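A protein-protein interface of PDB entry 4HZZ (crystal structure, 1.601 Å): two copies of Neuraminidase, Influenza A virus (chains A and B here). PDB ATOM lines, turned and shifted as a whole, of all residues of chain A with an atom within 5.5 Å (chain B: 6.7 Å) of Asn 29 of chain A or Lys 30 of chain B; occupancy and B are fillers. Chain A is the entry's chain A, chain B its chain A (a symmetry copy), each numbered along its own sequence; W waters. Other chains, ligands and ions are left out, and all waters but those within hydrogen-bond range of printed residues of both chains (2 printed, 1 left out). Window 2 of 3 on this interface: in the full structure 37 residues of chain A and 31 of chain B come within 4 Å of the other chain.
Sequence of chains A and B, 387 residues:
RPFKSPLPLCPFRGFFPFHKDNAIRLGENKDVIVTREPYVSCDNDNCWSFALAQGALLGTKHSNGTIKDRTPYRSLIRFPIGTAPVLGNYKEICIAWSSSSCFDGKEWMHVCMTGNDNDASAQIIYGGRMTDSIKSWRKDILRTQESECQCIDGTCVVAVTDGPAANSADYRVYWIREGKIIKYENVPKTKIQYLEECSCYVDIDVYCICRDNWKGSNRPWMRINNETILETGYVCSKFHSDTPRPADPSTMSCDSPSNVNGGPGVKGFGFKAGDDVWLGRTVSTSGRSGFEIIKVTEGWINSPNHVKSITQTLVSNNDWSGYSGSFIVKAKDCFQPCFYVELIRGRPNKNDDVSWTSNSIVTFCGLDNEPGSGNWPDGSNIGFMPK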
ATOM      1  N   LEU A  26      12.145 -31.885  26.928  1.00  0.00           N
ATOM      2  CA  LEU A  26      13.133 -30.826  27.164  1.00  0.00           C
ATOM      3  C   LEU A  26      14.144 -30.686  26.040  1.00  0.00           C
ATOM      4  O   LEU A  26      14.913 -29.722  26.009  1.00  0.00           O
ATOM      5  CB  LEU A  26      13.852 -31.066  28.494  1.00  0.00           C
ATOM      6  CG  LEU A  26      12.963 -30.829  29.713  1.00  0.00           C
ATOM      7  CD1 LEU A  26      13.591 -31.409  30.977  1.00  0.00           C
ATOM      8  CD2 LEU A  26      12.726 -29.315  29.907  1.00  0.00           C
ATOM      9  N   GLY A  27      14.139 -31.644  25.115  1.00  0.00           N
ATOM     10  CA  GLY A  27      15.079 -31.624  24.006  1.00  0.00           C
ATOM     11  C   GLY A  27      14.520 -31.015  22.737  1.00  0.00           C
ATOM     12  O   GLY A  27      15.153 -31.086  21.679  1.00  0.00           O
ATOM     13  N   GLU A  28      13.337 -30.415  22.833  1.00  0.00           N
ATOM     14  CA  GLU A  28      12.686 -29.841  21.655  1.00  0.00           C
ATOM     15  C   GLU A  28      13.539 -28.782  20.941  1.00  0.00           C
ATOM     16  O   GLU A  28      13.412 -28.594  19.732  1.00  0.00           O
ATOM     17  CB  GLU A  28      11.346 -29.216  22.059  1.00  0.00           C
ATOM     18  CG  GLU A  28      10.470 -28.833  20.891  1.00  0.00           C
ATOM     19  CD  GLU A  28       9.333 -27.925  21.314  1.00  0.00           C
ATOM     20  OE1 GLU A  28       8.709 -28.205  22.361  1.00  0.00           O
ATOM     21  OE2 GLU A  28       9.082 -26.928  20.603  1.00  0.00           O
ATOM     22  N   ASN A  29      14.396 -28.083  21.689  1.00  0.00           N
ATOM     23  CA  ASN A  29      15.231 -27.027  21.117  1.00  0.00           C
ATOM     24  C   ASN A  29      16.677 -27.477  20.898  1.00  0.00           C
ATOM     25  O   ASN A  29      17.583 -26.652  20.842  1.00  0.00           O
ATOM     26  CB  ASN A  29      15.182 -25.772  22.001  1.00  0.00           C
ATOM     27  CG  ASN A  29      15.489 -24.487  21.238  1.00  0.00           C
ATOM     28  OD1 ASN A  29      16.188 -23.607  21.749  1.00  0.00           O
ATOM     29  ND2 ASN A  29      14.966 -24.371  20.028  1.00  0.00           N
ATOM     30  N   LYS A  30      16.870 -28.792  20.793  1.00  0.00           N
ATOM     31  CA  LYS A  30      18.150 -29.407  20.411  1.00  0.00           C
ATOM     32  C   LYS A  30      19.260 -29.317  21.456  1.00  0.00           C
ATOM     33  O   LYS A  30      20.440 -29.376  21.110  1.00  0.00           O
ATOM     34  CB  LYS A  30      18.657 -28.857  19.069  1.00  0.00           C
ATOM     35  CG  LYS A  30      17.653 -28.992  17.944  1.00  0.00           C
ATOM     36  CD  LYS A  30      18.224 -28.470  16.643  1.00  0.00           C
ATOM     37  CE  LYS A  30      17.211 -28.574  15.533  1.00  0.00           C
ATOM     38  NZ  LYS A  30      17.645 -27.824  14.313  1.00  0.00           N
ATOM     39  N   ASP A  31      18.888 -29.226  22.728  1.00  0.00           N
ATOM     40  CA  ASP A  31      19.878 -29.181  23.805  1.00  0.00           C
ATOM     41  C   ASP A  31      20.310 -30.544  24.328  1.00  0.00           C
ATOM     42  O   ASP A  31      21.357 -30.655  24.953  1.00  0.00           O
ATOM     43  CB  ASP A  31      19.340 -28.377  24.992  1.00  0.00           C
ATOM     44  CG  ASP A  31      19.084 -26.930  24.638  1.00  0.00           C
ATOM     45  OD1 ASP A  31      20.058 -26.213  24.324  1.00  0.00           O
ATOM     46  OD2 ASP A  31      17.911 -26.513  24.661  1.00  0.00           O
ATOM     47  N   PRO A 386      11.902 -31.498  16.453  1.00  0.00           N
ATOM     48  CA  PRO A 386      12.746 -31.482  15.253  1.00  0.00           C
ATOM     49  C   PRO A 386      12.971 -32.926  14.810  1.00  0.00           C
ATOM     50  O   PRO A 386      13.221 -33.803  15.644  1.00  0.00           O
ATOM     51  CB  PRO A 386      14.055 -30.857  15.747  1.00  0.00           C
ATOM     52  CG  PRO A 386      14.028 -31.066  17.267  1.00  0.00           C
ATOM     53  CD  PRO A 386      12.585 -30.938  17.634  1.00  0.00           C
ATOM     54  N   LEU B  26      15.586 -13.618  30.980  1.00  0.00           N
ATOM     55  CA  LEU B  26      16.709 -14.458  30.547  1.00  0.00           C
ATOM     56  C   LEU B  26      16.278 -15.659  29.724  1.00  0.00           C
ATOM     57  O   LEU B  26      17.117 -16.345  29.135  1.00  0.00           O
ATOM     58  CB  LEU B  26      17.521 -14.915  31.762  1.00  0.00           C
ATOM     59  CG  LEU B  26      18.316 -13.787  32.416  1.00  0.00           C
ATOM     60  CD1 LEU B  26      18.817 -14.192  33.800  1.00  0.00           C
ATOM     61  CD2 LEU B  26      19.520 -13.405  31.527  1.00  0.00           C
ATOM     62  N   GLY B  27      14.971 -15.909  29.678  1.00  0.00           N
ATOM     63  CA  GLY B  27      14.447 -17.045  28.939  1.00  0.00           C
ATOM     64  C   GLY B  27      13.978 -16.706  27.539  1.00  0.00           C
ATOM     65  O   GLY B  27      13.363 -17.539  26.868  1.00  0.00           O
ATOM     66  N   GLU B  28      14.263 -15.486  27.093  1.00  0.00           N
ATOM     67  CA  GLU B  28      13.810 -15.040  25.775  1.00  0.00           C
ATOM     68  C   GLU B  28      14.296 -15.938  24.627  1.00  0.00           C
ATOM     69  O   GLU B  28      13.633 -16.040  23.595  1.00  0.00           O
ATOM     70  CB  GLU B  28      14.283 -13.605  25.524  1.00  0.00           C
ATOM     71  CG  GLU B  28      13.652 -12.952  24.318  1.00  0.00           C
ATOM     72  CD  GLU B  28      14.386 -11.689  23.913  1.00  0.00           C
ATOM     73  OE1 GLU B  28      14.735 -10.892  24.811  1.00  0.00           O
ATOM     74  OE2 GLU B  28      14.621 -11.511  22.699  1.00  0.00           O
ATOM     75  N   ASN B  29      15.456 -16.575  24.799  1.00  0.00           N
ATOM     76  CA  ASN B  29      16.027 -17.426  23.756  1.00  0.00           C
ATOM     77  C   ASN B  29      15.823 -18.917  24.037  1.00  0.00           C
ATOM     78  O   ASN B  29      16.568 -19.751  23.537  1.00  0.00           O
ATOM     79  CB  ASN B  29      17.519 -17.110  23.568  1.00  0.00           C
ATOM     80  CG  ASN B  29      18.038 -17.466  22.179  1.00  0.00           C
ATOM     81  OD1 ASN B  29      19.151 -17.983  22.040  1.00  0.00           O
ATOM     82  ND2 ASN B  29      17.247 -17.187  21.155  1.00  0.00           N
ATOM     83  N   LYS B  30      14.815 -19.223  24.855  1.00  0.00           N
ATOM     84  CA  LYS B  30      14.351 -20.595  25.110  1.00  0.00           C
ATOM     85  C   LYS B  30      15.299 -21.466  25.933  1.00  0.00           C
ATOM     86  O   LYS B  30      15.253 -22.693  25.834  1.00  0.00           O
ATOM     87  CB  LYS B  30      13.991 -21.316  23.802  1.00  0.00           C
ATOM     88  CG  LYS B  30      12.979 -20.568  22.961  1.00  0.00           C
ATOM     89  CD  LYS B  30      12.635 -21.346  21.708  1.00  0.00           C
ATOM     90  CE  LYS B  30      11.654 -20.583  20.857  1.00  0.00           C
ATOM     91  NZ  LYS B  30      11.507 -21.194  19.498  1.00  0.00           N
ATOM     92  N   ASP B  31      16.116 -20.844  26.775  1.00  0.00           N
ATOM     93  CA  ASP B  31      17.028 -21.594  27.640  1.00  0.00           C
ATOM     94  C   ASP B  31      16.434 -22.014  28.977  1.00  0.00           C
ATOM     95  O   ASP B  31      16.950 -22.921  29.617  1.00  0.00           O
ATOM     96  CB  ASP B  31      18.288 -20.774  27.928  1.00  0.00           C
ATOM     97  CG  ASP B  31      19.086 -20.486  26.677  1.00  0.00           C
ATOM     98  OD1 ASP B  31      19.598 -21.448  26.064  1.00  0.00           O
ATOM     99  OD2 ASP B  31      19.191 -19.305  26.299  1.00  0.00           O
ATOM    100  N   VAL B  32      15.348 -21.374  29.391  1.00  0.00           N
ATOM    101  CA  VAL B  32      14.902 -21.491  30.774  1.00  0.00           C
ATOM    102  C   VAL B  32      13.748 -22.490  30.932  1.00  0.00           C
ATOM    103  O   VAL B  32      12.844 -22.564  30.104  1.00  0.00           O
ATOM    104  CB  VAL B  32      14.539 -20.095  31.323  1.00  0.00           C
ATOM    105  CG1 VAL B  32      13.991 -20.175  32.749  1.00  0.00           C
ATOM    106  CG2 VAL B  32      15.768 -19.205  31.291  1.00  0.00           C
ATOM    107  N   ILE B  33      13.800 -23.273  32.003  1.00  0.00           N
ATOM    108  CA  ILE B  33      12.772 -24.254  32.292  1.00  0.00           C
ATOM    109  C   ILE B  33      11.505 -23.555  32.788  1.00  0.00           C
ATOM    110  O   ILE B  33      11.583 -22.640  33.607  1.00  0.00           O
ATOM    111  CB  ILE B  33      13.291 -25.235  33.357  1.00  0.00           C
ATOM    112  CG1 ILE B  33      14.553 -25.944  32.841  1.00  0.00           C
ATOM    113  CG2 ILE B  33      12.230 -26.267  33.710  1.00  0.00           C
ATOM    114  CD1 ILE B  33      15.346 -26.670  33.922  1.00  0.00           C
ATOM    115  N   LEU B  57      10.847 -26.330  28.156  1.00  0.00           N
ATOM    116  CA  LEU B  57      11.549 -25.051  28.123  1.00  0.00           C
ATOM    117  C   LEU B  57      10.605 -23.928  27.691  1.00  0.00           C
ATOM    118  O   LEU B  57       9.756 -24.104  26.817  1.00  0.00           O
ATOM    119  CB  LEU B  57      12.768 -25.110  27.188  1.00  0.00           C
ATOM    120  CG  LEU B  57      13.841 -26.131  27.565  1.00  0.00           C
ATOM    121  CD1 LEU B  57      14.980 -26.105  26.555  1.00  0.00           C
ATOM    122  CD2 LEU B  57      14.375 -25.911  28.986  1.00  0.00           C
ATOM    123  N   LEU B  58      10.783 -22.765  28.298  1.00  0.00           N
ATOM    124  CA  LEU B  58       9.923 -21.610  28.046  1.00  0.00           C
ATOM    125  C   LEU B  58      10.004 -21.180  26.584  1.00  0.00           C
ATOM    126  O   LEU B  58      11.094 -20.973  26.059  1.00  0.00           O
ATOM    127  CB  LEU B  58      10.358 -20.465  28.964  1.00  0.00           C
ATOM    128  CG  LEU B  58       9.609 -19.132  28.964  1.00  0.00           C
ATOM    129  CD1 LEU B  58       8.358 -19.248  29.765  1.00  0.00           C
ATOM    130  CD2 LEU B  58      10.518 -18.064  29.580  1.00  0.00           C
ATOM    131  N   GLY B  59       8.848 -21.058  25.928  1.00  0.00           N
ATOM    132  CA  GLY B  59       8.805 -20.604  24.549  1.00  0.00           C
ATOM    133  C   GLY B  59       8.839 -21.717  23.512  1.00  0.00           C
ATOM    134  O   GLY B  59       8.749 -21.459  22.307  1.00  0.00           O
ATOM    135  N   THR B  60       9.015 -22.956  23.965  1.00  0.00           N
ATOM    136  CA  THR B  60       8.944 -24.101  23.056  1.00  0.00           C
ATOM    137  C   THR B  60       7.489 -24.523  22.929  1.00  0.00           C
ATOM    138  O   THR B  60       6.625 -24.044  23.665  1.00  0.00           O
ATOM    139  CB  THR B  60       9.811 -25.293  23.533  1.00  0.00           C
ATOM    140  OG1 THR B  60       9.301 -25.802  24.770  1.00  0.00           O
ATOM    141  CG2 THR B  60      11.268 -24.859  23.708  1.00  0.00           C
ATOM    142  N   LYS B  61       7.203 -25.381  21.959  1.00  0.00           N
ATOM    143  CA  LYS B  61       5.826 -25.818  21.748  1.00  0.00           C
ATOM    144  C   LYS B  61       5.298 -26.587  22.954  1.00  0.00           C
ATOM    145  O   LYS B  61       4.110 -26.513  23.283  1.00  0.00           O
ATOM    146  CB  LYS B  61       5.729 -26.659  20.468  1.00  0.00           C
ATOM    147  CG  LYS B  61       6.040 -25.884  19.191  1.00  0.00           C
ATOM    148  CD  LYS B  61       5.989 -26.798  17.993  1.00  0.00           C
ATOM    149  CE  LYS B  61       6.144 -26.015  16.692  1.00  0.00           C
ATOM    150  NZ  LYS B  61       7.562 -25.614  16.478  1.00  0.00           N
ATOM    151  N   PRO B 386       9.085 -15.429  22.957  1.00  0.00           N
ATOM    152  CA  PRO B 386       8.482 -16.491  22.143  1.00  0.00           C
ATOM    153  C   PRO B 386       7.167 -16.906  22.800  1.00  0.00           C
ATOM    154  O   PRO B 386       7.100 -17.050  24.025  1.00  0.00           O
ATOM    155  CB  PRO B 386       9.508 -17.626  22.222  1.00  0.00           C
ATOM    156  CG  PRO B 386      10.326 -17.313  23.482  1.00  0.00           C
ATOM    157  CD  PRO B 386      10.388 -15.821  23.524  1.00  0.00           C
ATOM    158  N   LYS B 387       6.128 -17.083  21.996  1.00  0.00           N
ATOM    159  CA  LYS B 387       4.796 -17.325  22.532  1.00  0.00           C
ATOM    160  C   LYS B 387       4.525 -18.789  22.877  1.00  0.00           C
ATOM    161  O   LYS B 387       5.286 -19.691  22.527  1.00  0.00           O
ATOM    162  CB  LYS B 387       3.738 -16.788  21.561  1.00  0.00           C
ATOM    163  CG  LYS B 387       3.784 -15.261  21.429  1.00  0.00           C
ATOM    164  CD  LYS B 387       2.678 -14.738  20.511  1.00  0.00           C
ATOM    165  CE  LYS B 387       2.831 -13.245  20.231  1.00  0.00           C
ATOM    166  NZ  LYS B 387       2.840 -12.408  21.462  1.00  0.00           N
ATOM    167  OXT LYS B 387       3.533 -19.101  23.534  1.00  0.00           O
HETATM  168  O   HOH W   1      10.097 -26.084  18.335  1.00  0.00           O
HETATM  169  O   HOH W   2      16.864 -20.866  20.969  1.00  0.00           O
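Printed residues of chain B within 4 Å of Leu 26 of chain A: Leu 57. Asn 29 of chain A touches just one residue of chain B: Lys 30. Printed residues of chain B within 4 Å of Asp 31 of chain A: Leu 57 (3.5 Å). Of chain A, only Asn 29 comes within 4 Å of Lys 30 of chain B. Of the printed residues of chain A, Leu 57 of chain B touches Leu 26 and Asp 31. Of the printed residues of chain A, Lys 61 of chain B touches Glu 28. Lys 387 of chain B touches none of the printed residues of chain A. The nearest residue of chain A that does not touch Lys 30 of chain B is Asp 31 of chain A (4.8 Å).
Water W1 lies within hydrogen-bond range of OE2 of Glu 28 of chain A (2.6 Å) and NZ of Lys 61 of chain B (3.2 Å). Water W2 bridges the backbone carbonyl oxygen of Asn 29 of chain B (2.8 Å) and the side-chain amide oxygen of Asn 29 of chain A (2.9 Å).
The backbone carbonyl oxygen (O) of Leu 57 of chain B sits at hydrogen-bond distance from the side-chain hydroxyl (OG1) of Thr 60 of chain B (2.7 Å).
Asn 29 of chain A touches Lys 30 of chain B, but with the chains exchanged Lys 30 of chain A does not touch Asn 29 of chain B (9.5 Å). Positions printed for both chains: 26, 27, 28, 29, 30, 31 and 386.
Printed residues of chain B that touch a printed residue of chain A: Lys 30, Leu 57, Thr 60 and Lys 61. Hydrophobic or aromatic side chains of chain B within 4 Å of the printed part of chain A: Leu 57. Hydrophobic or aromatic side chains of chain A that line the printed part of chain B: Leu 26.
OE1 of Glu 28 of chain A sits close to OG1 of Thr 60 of chain B (3.5 Å). OE2 of Glu 28 of chain A sits at hydrogen-bond distance from N of Lys 61 of chain B, at 2.8 Å.
Leu 26 of chain A touches Leu 57 of chain B (O to CD1, 3.7 Å). OD1 of Asn 29 of chain A touches CB of Lys 30 of chain B, at 3.8 Å. Asp 31 of chain A touches Leu 57 of chain B (OD2 to CD1, 3.5 Å).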
